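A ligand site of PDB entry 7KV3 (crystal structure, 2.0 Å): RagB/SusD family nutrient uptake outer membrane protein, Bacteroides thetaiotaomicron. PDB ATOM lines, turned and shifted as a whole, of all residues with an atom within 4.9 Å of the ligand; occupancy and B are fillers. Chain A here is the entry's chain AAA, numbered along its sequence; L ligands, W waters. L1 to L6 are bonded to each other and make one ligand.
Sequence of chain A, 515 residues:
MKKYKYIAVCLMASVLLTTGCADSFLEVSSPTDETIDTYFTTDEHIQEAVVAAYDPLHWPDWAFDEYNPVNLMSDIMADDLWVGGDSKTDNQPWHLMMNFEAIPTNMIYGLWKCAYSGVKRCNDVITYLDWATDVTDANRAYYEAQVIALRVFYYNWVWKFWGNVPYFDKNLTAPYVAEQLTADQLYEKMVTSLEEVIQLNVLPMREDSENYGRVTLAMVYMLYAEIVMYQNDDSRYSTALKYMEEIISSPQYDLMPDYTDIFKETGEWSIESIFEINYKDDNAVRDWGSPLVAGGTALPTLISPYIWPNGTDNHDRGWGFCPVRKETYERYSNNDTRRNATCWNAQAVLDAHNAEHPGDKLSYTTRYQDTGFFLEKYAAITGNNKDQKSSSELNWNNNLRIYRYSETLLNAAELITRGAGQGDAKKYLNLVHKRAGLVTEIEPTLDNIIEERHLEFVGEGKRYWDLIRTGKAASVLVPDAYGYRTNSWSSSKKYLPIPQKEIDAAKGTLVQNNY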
ATOM      1  N   TRP A  62     -19.235 -10.418 -13.496  1.00  0.00           N
ATOM      2  CA  TRP A  62     -18.457 -10.934 -12.322  1.00  0.00           C
ATOM      3  C   TRP A  62     -16.990 -11.104 -12.734  1.00  0.00           C
ATOM      4  O   TRP A  62     -16.672 -12.106 -13.426  1.00  0.00           O
ATOM      5  CB  TRP A  62     -19.019 -12.219 -11.732  1.00  0.00           C
ATOM      6  CG  TRP A  62     -18.158 -12.772 -10.635  1.00  0.00           C
ATOM      7  CD1 TRP A  62     -17.464 -13.957 -10.675  1.00  0.00           C
ATOM      8  CD2 TRP A  62     -17.808 -12.164  -9.384  1.00  0.00           C
ATOM      9  NE1 TRP A  62     -16.773 -14.143  -9.508  1.00  0.00           N
ATOM     10  CE2 TRP A  62     -16.934 -13.051  -8.707  1.00  0.00           C
ATOM     11  CE3 TRP A  62     -18.175 -10.969  -8.736  1.00  0.00           C
ATOM     12  CZ2 TRP A  62     -16.424 -12.789  -7.429  1.00  0.00           C
ATOM     13  CZ3 TRP A  62     -17.665 -10.705  -7.480  1.00  0.00           C
ATOM     14  CH2 TRP A  62     -16.801 -11.612  -6.829  1.00  0.00           C
ATOM     15  N   ASP A  65     -13.214  -9.256  -8.851  1.00  0.00           N
ATOM     16  CA  ASP A  65     -13.891  -9.204  -7.540  1.00  0.00           C
ATOM     17  C   ASP A  65     -15.017  -8.156  -7.507  1.00  0.00           C
ATOM     18  O   ASP A  65     -15.326  -7.701  -6.396  1.00  0.00           O
ATOM     19  CB  ASP A  65     -12.876  -8.921  -6.429  1.00  0.00           C
ATOM     20  CG  ASP A  65     -13.378  -9.303  -5.056  1.00  0.00           C
ATOM     21  OD1 ASP A  65     -14.221 -10.209  -4.988  1.00  0.00           O
ATOM     22  OD2 ASP A  65     -12.936  -8.675  -4.060  1.00  0.00           O
ATOM     23  N   TYR A  67     -19.110  -6.976  -9.386  1.00  0.00           N
ATOM     24  CA  TYR A  67     -20.316  -7.095 -10.256  1.00  0.00           C
ATOM     25  C   TYR A  67     -20.455  -5.768 -11.012  1.00  0.00           C
ATOM     26  O   TYR A  67     -20.829  -4.796 -10.390  1.00  0.00           O
ATOM     27  CB  TYR A  67     -21.559  -7.358  -9.409  1.00  0.00           C
ATOM     28  CG  TYR A  67     -21.494  -8.543  -8.483  1.00  0.00           C
ATOM     29  CD1 TYR A  67     -21.726  -9.817  -8.960  1.00  0.00           C
ATOM     30  CD2 TYR A  67     -21.236  -8.399  -7.131  1.00  0.00           C
ATOM     31  CE1 TYR A  67     -21.666 -10.912  -8.127  1.00  0.00           C
ATOM     32  CE2 TYR A  67     -21.156  -9.491  -6.284  1.00  0.00           C
ATOM     33  CZ  TYR A  67     -21.364 -10.755  -6.783  1.00  0.00           C
ATOM     34  OH  TYR A  67     -21.347 -11.884  -6.002  1.00  0.00           O
ATOM     35  N   ASP A  90     -24.705  -1.948   0.043  1.00  0.00           N
ATOM     36  CA  ASP A  90     -24.612  -3.199  -0.753  1.00  0.00           C
ATOM     37  C   ASP A  90     -24.300  -2.818  -2.220  1.00  0.00           C
ATOM     38  O   ASP A  90     -25.141  -2.180  -2.844  1.00  0.00           O
ATOM     39  CB  ASP A  90     -25.892  -4.030  -0.575  1.00  0.00           C
ATOM     40  CG  ASP A  90     -25.720  -5.493  -0.941  1.00  0.00           C
ATOM     41  OD1 ASP A  90     -24.588  -5.878  -1.325  1.00  0.00           O
ATOM     42  OD2 ASP A  90     -26.742  -6.234  -0.898  1.00  0.00           O
ATOM     43  N   ASN A  91     -23.132  -3.207  -2.758  1.00  0.00           N
ATOM     44  CA  ASN A  91     -22.601  -2.685  -4.052  1.00  0.00           C
ATOM     45  C   ASN A  91     -22.668  -1.146  -3.979  1.00  0.00           C
ATOM     46  O   ASN A  91     -23.319  -0.538  -4.828  1.00  0.00           O
ATOM     47  CB  ASN A  91     -23.351  -3.242  -5.277  1.00  0.00           C
ATOM     48  CG  ASN A  91     -22.930  -4.650  -5.670  1.00  0.00           C
ATOM     49  OD1 ASN A  91     -21.746  -4.999  -5.614  1.00  0.00           O
ATOM     50  ND2 ASN A  91     -23.870  -5.459  -6.130  1.00  0.00           N
ATOM     51  N   VAL A 285     -18.952 -23.755 -16.026  1.00  0.00           N
ATOM     52  CA  VAL A 285     -18.123 -23.932 -14.791  1.00  0.00           C
ATOM     53  C   VAL A 285     -17.476 -22.606 -14.401  1.00  0.00           C
ATOM     54  O   VAL A 285     -16.459 -22.630 -13.681  1.00  0.00           O
ATOM     55  CB  VAL A 285     -17.068 -25.057 -14.944  1.00  0.00           C
ATOM     56  CG1 VAL A 285     -17.706 -26.433 -14.850  1.00  0.00           C
ATOM     57  CG2 VAL A 285     -16.269 -24.931 -16.240  1.00  0.00           C
ATOM     58  N   ASP A 287     -16.885 -19.794 -11.931  1.00  0.00           N
ATOM     59  CA  ASP A 287     -16.907 -19.895 -10.457  1.00  0.00           C
ATOM     60  C   ASP A 287     -16.328 -18.604  -9.850  1.00  0.00           C
ATOM     61  O   ASP A 287     -15.781 -17.751 -10.602  1.00  0.00           O
ATOM     62  CB  ASP A 287     -16.220 -21.187 -10.006  1.00  0.00           C
ATOM     63  CG  ASP A 287     -16.786 -21.820  -8.729  1.00  0.00           C
ATOM     64  OD1 ASP A 287     -17.643 -21.187  -8.075  1.00  0.00           O
ATOM     65  OD2 ASP A 287     -16.355 -22.923  -8.399  1.00  0.00           O
ATOM     66  N   TRP A 288     -16.520 -18.446  -8.543  1.00  0.00           N
ATOM     67  CA  TRP A 288     -16.119 -17.243  -7.765  1.00  0.00           C
ATOM     68  C   TRP A 288     -14.630 -16.944  -7.938  1.00  0.00           C
ATOM     69  O   TRP A 288     -14.304 -15.758  -8.160  1.00  0.00           O
ATOM     70  CB  TRP A 288     -16.520 -17.421  -6.288  1.00  0.00           C
ATOM     71  CG  TRP A 288     -17.976 -17.713  -6.150  1.00  0.00           C
ATOM     72  CD1 TRP A 288     -18.558 -18.928  -5.947  1.00  0.00           C
ATOM     73  CD2 TRP A 288     -19.060 -16.772  -6.283  1.00  0.00           C
ATOM     74  NE1 TRP A 288     -19.916 -18.805  -5.902  1.00  0.00           N
ATOM     75  CE2 TRP A 288     -20.255 -17.496  -6.115  1.00  0.00           C
ATOM     76  CE3 TRP A 288     -19.124 -15.383  -6.516  1.00  0.00           C
ATOM     77  CZ2 TRP A 288     -21.509 -16.884  -6.159  1.00  0.00           C
ATOM     78  CZ3 TRP A 288     -20.364 -14.796  -6.603  1.00  0.00           C
ATOM     79  CH2 TRP A 288     -21.532 -15.537  -6.419  1.00  0.00           C
ATOM     80  N   SER A 290     -12.703 -18.396 -10.380  1.00  0.00           N
ATOM     81  CA  SER A 290     -12.412 -18.541 -11.835  1.00  0.00           C
ATOM     82  C   SER A 290     -13.491 -17.813 -12.640  1.00  0.00           C
ATOM     83  O   SER A 290     -14.295 -18.380 -13.398  1.00  0.00           O
ATOM     84  CB  SER A 290     -12.274 -19.992 -12.213  1.00  0.00           C
ATOM     85  OG  SER A 290     -13.461 -20.708 -11.941  1.00  0.00           O
ATOM     86  N   TRP A 319     -30.877 -11.424  -5.493  1.00  0.00           N
ATOM     87  CA  TRP A 319     -30.428 -10.529  -4.394  1.00  0.00           C
ATOM     88  C   TRP A 319     -31.204  -9.195  -4.399  1.00  0.00           C
ATOM     89  O   TRP A 319     -30.843  -8.314  -3.634  1.00  0.00           O
ATOM     90  CB  TRP A 319     -28.908 -10.347  -4.478  1.00  0.00           C
ATOM     91  CG  TRP A 319     -28.109 -11.607  -4.226  1.00  0.00           C
ATOM     92  CD1 TRP A 319     -28.423 -12.662  -3.417  1.00  0.00           C
ATOM     93  CD2 TRP A 319     -26.818 -11.923  -4.770  1.00  0.00           C
ATOM     94  NE1 TRP A 319     -27.425 -13.610  -3.447  1.00  0.00           N
ATOM     95  CE2 TRP A 319     -26.424 -13.177  -4.263  1.00  0.00           C
ATOM     96  CE3 TRP A 319     -25.950 -11.265  -5.641  1.00  0.00           C
ATOM     97  CZ2 TRP A 319     -25.229 -13.797  -4.598  1.00  0.00           C
ATOM     98  CZ3 TRP A 319     -24.745 -11.851  -5.954  1.00  0.00           C
ATOM     99  CH2 TRP A 319     -24.394 -13.104  -5.443  1.00  0.00           C
ATOM    100  N   PHE A 321     -31.496  -6.632  -6.517  1.00  0.00           N
ATOM    101  CA  PHE A 321     -30.950  -5.413  -7.142  1.00  0.00           C
ATOM    102  C   PHE A 321     -31.847  -5.006  -8.314  1.00  0.00           C
ATOM    103  O   PHE A 321     -32.591  -5.847  -8.828  1.00  0.00           O
ATOM    104  CB  PHE A 321     -29.493  -5.603  -7.578  1.00  0.00           C
ATOM    105  CG  PHE A 321     -28.501  -5.590  -6.444  1.00  0.00           C
ATOM    106  CD1 PHE A 321     -27.962  -4.400  -5.974  1.00  0.00           C
ATOM    107  CD2 PHE A 321     -28.091  -6.770  -5.861  1.00  0.00           C
ATOM    108  CE1 PHE A 321     -27.037  -4.395  -4.944  1.00  0.00           C
ATOM    109  CE2 PHE A 321     -27.153  -6.780  -4.833  1.00  0.00           C
ATOM    110  CZ  PHE A 321     -26.637  -5.584  -4.366  1.00  0.00           C
ATOM    111  N   ARG A 367     -36.328  -6.078  -0.215  1.00  0.00           N
ATOM    112  CA  ARG A 367     -35.030  -5.437   0.075  1.00  0.00           C
ATOM    113  C   ARG A 367     -35.191  -3.945  -0.177  1.00  0.00           C
ATOM    114  O   ARG A 367     -36.294  -3.492  -0.361  1.00  0.00           O
ATOM    115  CB  ARG A 367     -33.923  -6.149  -0.729  1.00  0.00           C
ATOM    116  CG  ARG A 367     -33.166  -7.203   0.091  1.00  0.00           C
ATOM    117  CD  ARG A 367     -31.970  -7.789  -0.632  1.00  0.00           C
ATOM    118  NE  ARG A 367     -31.028  -8.412   0.299  1.00  0.00           N
ATOM    119  CZ  ARG A 367     -29.805  -8.817  -0.016  1.00  0.00           C
ATOM    120  NH1 ARG A 367     -29.363  -8.698  -1.257  1.00  0.00           N
ATOM    121  NH2 ARG A 367     -29.028  -9.372   0.906  1.00  0.00           N
ATOM    122  N   LYS A 389     -22.377 -26.783 -13.874  1.00  0.00           N
ATOM    123  CA  LYS A 389     -21.595 -27.817 -13.133  1.00  0.00           C
ATOM    124  C   LYS A 389     -20.727 -27.147 -12.063  1.00  0.00           C
ATOM    125  O   LYS A 389     -19.899 -27.863 -11.461  1.00  0.00           O
ATOM    126  CB  LYS A 389     -20.764 -28.669 -14.100  1.00  0.00           C
ATOM    127  CG  LYS A 389     -21.596 -29.510 -15.060  1.00  0.00           C
ATOM    128  CD  LYS A 389     -22.212 -30.741 -14.418  1.00  0.00           C
ATOM    129  CE  LYS A 389     -23.675 -30.940 -14.764  1.00  0.00           C
ATOM    130  NZ  LYS A 389     -23.837 -31.673 -16.035  1.00  0.00           N
ATOM    131  N   SER A 390     -20.950 -25.857 -11.792  1.00  0.00           N
ATOM    132  CA  SER A 390     -20.210 -25.112 -10.735  1.00  0.00           C
ATOM    133  C   SER A 390     -21.182 -24.433  -9.756  1.00  0.00           C
ATOM    134  O   SER A 390     -22.119 -25.119  -9.288  1.00  0.00           O
ATOM    135  CB  SER A 390     -19.267 -24.153 -11.383  1.00  0.00           C
ATOM    136  OG  SER A 390     -18.307 -23.738 -10.433  1.00  0.00           O
ATOM    137  N   SER A 391     -20.968 -23.156  -9.436  1.00  0.00           N
ATOM    138  CA  SER A 391     -21.887 -22.313  -8.609  1.00  0.00           C
ATOM    139  C   SER A 391     -23.008 -21.764  -9.502  1.00  0.00           C
ATOM    140  O   SER A 391     -22.708 -20.941 -10.418  1.00  0.00           O
ATOM    141  CB  SER A 391     -21.109 -21.245  -7.906  1.00  0.00           C
ATOM    142  OG  SER A 391     -19.936 -21.817  -7.331  1.00  0.00           O
ATOM    143  N   GLU A 393     -25.244 -19.638  -9.231  1.00  0.00           N
ATOM    144  CA  GLU A 393     -25.370 -18.166  -9.166  1.00  0.00           C
ATOM    145  C   GLU A 393     -24.714 -17.486 -10.366  1.00  0.00           C
ATOM    146  O   GLU A 393     -25.181 -16.399 -10.734  1.00  0.00           O
ATOM    147  CB  GLU A 393     -24.657 -17.561  -7.949  1.00  0.00           C
ATOM    148  CG  GLU A 393     -25.418 -17.761  -6.662  1.00  0.00           C
ATOM    149  CD  GLU A 393     -25.104 -19.058  -5.943  1.00  0.00           C
ATOM    150  OE1 GLU A 393     -24.171 -19.773  -6.368  1.00  0.00           O
ATOM    151  OE2 GLU A 393     -25.792 -19.362  -4.943  1.00  0.00           O
HETATM  152  C1  LIG L   1     -15.173 -25.523 -10.409  1.00  0.00           C
HETATM  153  C2  LIG L   1     -15.984 -26.517  -9.595  1.00  0.00           C
HETATM  154  C3  LIG L   1     -16.497 -27.626 -10.538  1.00  0.00           C
HETATM  155  C4  LIG L   1     -15.398 -28.199 -11.434  1.00  0.00           C
HETATM  156  C5  LIG L   1     -16.038 -29.010 -12.535  1.00  0.00           C
HETATM  157  C6  LIG L   1     -14.010 -26.317 -11.021  1.00  0.00           C
HETATM  158  O1  LIG L   1     -13.144 -25.404 -11.642  1.00  0.00           O
HETATM  159  O2  LIG L   1     -14.704 -24.454  -9.583  1.00  0.00           O
HETATM  160  O3  LIG L   1     -17.072 -25.853  -8.918  1.00  0.00           O
HETATM  161  O4  LIG L   1     -17.114 -28.715  -9.839  1.00  0.00           O
HETATM  162  O5  LIG L   1     -14.546 -27.182 -12.007  1.00  0.00           O
HETATM  163  O6  LIG L   1     -14.965 -29.338 -13.399  1.00  0.00           O
HETATM  164  C1  LG2 L   2     -18.233 -25.202  -6.995  1.00  0.00           C
HETATM  165  C2  LG2 L   2     -19.064 -25.747  -5.868  1.00  0.00           C
HETATM  166  C3  LG2 L   2     -20.079 -26.751  -6.422  1.00  0.00           C
HETATM  167  C4  LG2 L   2     -19.388 -27.846  -7.231  1.00  0.00           C
HETATM  168  C5  LG2 L   2     -20.393 -28.811  -7.808  1.00  0.00           C
HETATM  169  C6  LG2 L   2     -17.667 -26.354  -7.833  1.00  0.00           C
HETATM  170  O1  LG2 L   2     -17.216 -24.345  -6.453  1.00  0.00           O
HETATM  171  O2  LG2 L   2     -19.747 -24.647  -5.270  1.00  0.00           O
HETATM  172  O3  LG2 L   2     -20.847 -27.326  -5.366  1.00  0.00           O
HETATM  173  O4  LG2 L   2     -18.670 -27.247  -8.306  1.00  0.00           O
HETATM  174  O5  LG2 L   2     -19.696 -29.974  -8.224  1.00  0.00           O
HETATM  175  C1  LG3 L   3     -19.853 -22.840  -3.861  1.00  0.00           C
HETATM  176  C2  LG3 L   3     -19.666 -22.504  -2.383  1.00  0.00           C
HETATM  177  C3  LG3 L   3     -20.562 -23.427  -1.565  1.00  0.00           C
HETATM  178  C4  LG3 L   3     -20.290 -24.913  -1.876  1.00  0.00           C
HETATM  179  C5  LG3 L   3     -21.478 -25.708  -1.293  1.00  0.00           C
HETATM  180  C6  LG3 L   3     -19.302 -24.258  -4.072  1.00  0.00           C
HETATM  181  O1  LG3 L   3     -19.201 -21.917  -4.732  1.00  0.00           O
HETATM  182  O2  LG3 L   3     -20.010 -21.146  -2.127  1.00  0.00           O
HETATM  183  O3  LG3 L   3     -20.434 -23.192  -0.152  1.00  0.00           O
HETATM  184  O4  LG3 L   3     -20.117 -25.197  -3.300  1.00  0.00           O
HETATM  185  O5  LG3 L   3     -21.116 -27.089  -1.215  1.00  0.00           O
HETATM  186  C1  LG4 L   4     -20.248 -18.737  -2.201  1.00  0.00           C
HETATM  187  C2  LG4 L   4     -19.355 -17.505  -2.206  1.00  0.00           C
HETATM  188  C3  LG4 L   4     -18.078 -17.735  -1.416  1.00  0.00           C
HETATM  189  C4  LG4 L   4     -17.435 -19.047  -1.813  1.00  0.00           C
HETATM  190  C5  LG4 L   4     -16.136 -19.211  -1.057  1.00  0.00           C
HETATM  191  C6  LG4 L   4     -19.411 -20.003  -2.396  1.00  0.00           C
HETATM  192  O1  LG4 L   4     -21.267 -18.653  -3.216  1.00  0.00           O
HETATM  193  O2  LG4 L   4     -20.045 -16.378  -1.654  1.00  0.00           O
HETATM  194  O3  LG4 L   4     -17.182 -16.657  -1.704  1.00  0.00           O
HETATM  195  O4  LG4 L   4     -18.315 -20.098  -1.505  1.00  0.00           O
HETATM  196  O5  LG4 L   4     -15.269 -18.379  -1.792  1.00  0.00           O
HETATM  197  C1  LG5 L   5     -21.451 -14.593  -1.504  1.00  0.00           C
HETATM  198  C2  LG5 L   5     -21.839 -13.278  -2.134  1.00  0.00           C
HETATM  199  C3  LG5 L   5     -20.613 -12.503  -2.607  1.00  0.00           C
HETATM  200  C4  LG5 L   5     -19.740 -13.428  -3.443  1.00  0.00           C
HETATM  201  C5  LG5 L   5     -18.487 -12.709  -3.914  1.00  0.00           C
HETATM  202  C6  LG5 L   5     -20.523 -15.401  -2.439  1.00  0.00           C
HETATM  203  O1  LG5 L   5     -22.584 -15.397  -1.341  1.00  0.00           O
HETATM  204  O2  LG5 L   5     -22.540 -12.451  -1.221  1.00  0.00           O
HETATM  205  O3  LG5 L   5     -21.043 -11.375  -3.367  1.00  0.00           O
HETATM  206  O4  LG5 L   5     -19.377 -14.599  -2.715  1.00  0.00           O
HETATM  207  O5  LG5 L   5     -17.635 -12.386  -2.807  1.00  0.00           O
HETATM  208  C1  LG6 L   6     -24.473 -11.482  -0.247  1.00  0.00           C
HETATM  209  C2  LG6 L   6     -25.724 -10.681  -0.593  1.00  0.00           C
HETATM  210  C3  LG6 L   6     -25.308  -9.490  -1.414  1.00  0.00           C
HETATM  211  C4  LG6 L   6     -24.492  -9.943  -2.646  1.00  0.00           C
HETATM  212  C5  LG6 L   6     -23.980  -8.792  -3.526  1.00  0.00           C
HETATM  213  C6  LG6 L   6     -23.708 -11.871  -1.485  1.00  0.00           C
HETATM  214  O1  LG6 L   6     -24.853 -12.709   0.363  1.00  0.00           O
HETATM  215  O2  LG6 L   6     -26.385 -10.331   0.626  1.00  0.00           O
HETATM  216  O3  LG6 L   6     -26.481  -8.805  -1.796  1.00  0.00           O
HETATM  217  O4  LG6 L   6     -23.375 -10.701  -2.195  1.00  0.00           O
HETATM  218  O5  LG6 L   6     -23.454  -7.722  -2.732  1.00  0.00           O
HETATM  219  O   HOH W   1     -20.932  -6.884  -3.669  1.00  0.00           O
HETATM  220  O   HOH W   2     -16.533 -21.460  -4.674  1.00  0.00           O
HETATM  221  O   HOH W   3     -22.381 -20.459  -4.658  1.00  0.00           O
HETATM  222  O   HOH W   4     -14.036 -23.203 -13.181  1.00  0.00           O
HETATM  223  O   HOH W   5     -21.276  -9.075  -0.226  1.00  0.00           O
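CH2 of Trp 62 touches C5 of LG5 L5, at 3.5 Å.
CG1 of Val 285 touches C5 of LIG L1, 3.8 Å away.
CE3 of Trp 319 touches C4 of LG6 L6, 3.6 Å away.
CE2 of Phe 321 touches O3 of LG6 L6 (3.7 Å).
Hydrophobic or aromatic side chains that line the ligand: Trp 62, Tyr 67, Val 285, Trp 288, Trp 319 and Phe 321.
12 residues have an atom within 4 Å of the ligand: Trp 62, Tyr 67, Asp 90, Val 285, Asp 287, Trp 288, Trp 319, Phe 321, Arg 367, Lys 389, Ser 390 and Ser 391.
The nearest printed residue that does not touch the ligand is Asn 91 (4.1 Å).
Water W3 lies within hydrogen-bond range of an oxygen (O1) of LG4 L4 (2.6 Å), the side-chain carboxylate (OE1) of Glu 393 (2.6 Å) and the indole nitrogen (NE1) of Trp 288 (3.2 Å).
Water W1 lies within hydrogen-bond range of O5 of LG6 L6 (2.8 Å) and OD1 of Asn 91 (2.8 Å).
Water W4 lies within hydrogen-bond range of O of Val 285 (2.5 Å), O1 of LIG L1 (2.8 Å) and OG of Ser 290 (2.8 Å).
The backbone carbonyl oxygen of Trp 288 lies within hydrogen-bond range of the indole nitrogen of Trp 62, 3.2 Å away.
The side-chain hydroxyl (OG) of Ser 390 lies within hydrogen-bond range of the side-chain carboxylate (OD2) of Asp 287 (2.9 Å).
The guanidinium group of Arg 367 sits at hydrogen-bond distance from the backbone carbonyl oxygen of Trp 319 (2.8 Å).
The side-chain carboxylate (OD1) of Asp 287 lies within hydrogen-bond range of the side-chain hydroxyl (OG) of Ser 391, 2.5 Å away.
The side-chain hydroxyl (OG) of Ser 391 lies within hydrogen-bond range of the indole nitrogen (NE1) of Trp 288 (3.3 Å).
OD2 of Asp 90 lies within salt-bridge range of NH1 of Arg 367 (3.6 Å).
The side-chain carboxylate (OD1) of Asp 90 sits at hydrogen-bond distance from an oxygen (O5) of LG6 L6, 2.6 Å away.
The indole nitrogen (NE1) of Trp 288 sits at hydrogen-bond distance from an oxygen (O1) of LG4 L4, 3.0 Å away.
OG of Ser 390 sits at hydrogen-bond distance from O3 of LIG L1.
An oxygen (O4) of LIG L1 is in hydrogen-bond range of the backbone carbonyl oxygen (O) of Lys 389 (3.3 Å).
The side-chain carboxylate of Asp 287 is in hydrogen-bond range of an oxygen (O2) of LIG L1, 2.5 Å away.
The side-chain hydroxyl (OH) of Tyr 67 sits at hydrogen-bond distance from an oxygen (O3) of LG5 L5.
The guanidinium group (NH2) of Arg 367 is in hydrogen-bond range of an oxygen (O2) of LG6 L6.
An oxygen (O1) of LG3 L3 is in hydrogen-bond range of the side-chain hydroxyl (OG) of Ser 391, at 2.7 Å.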
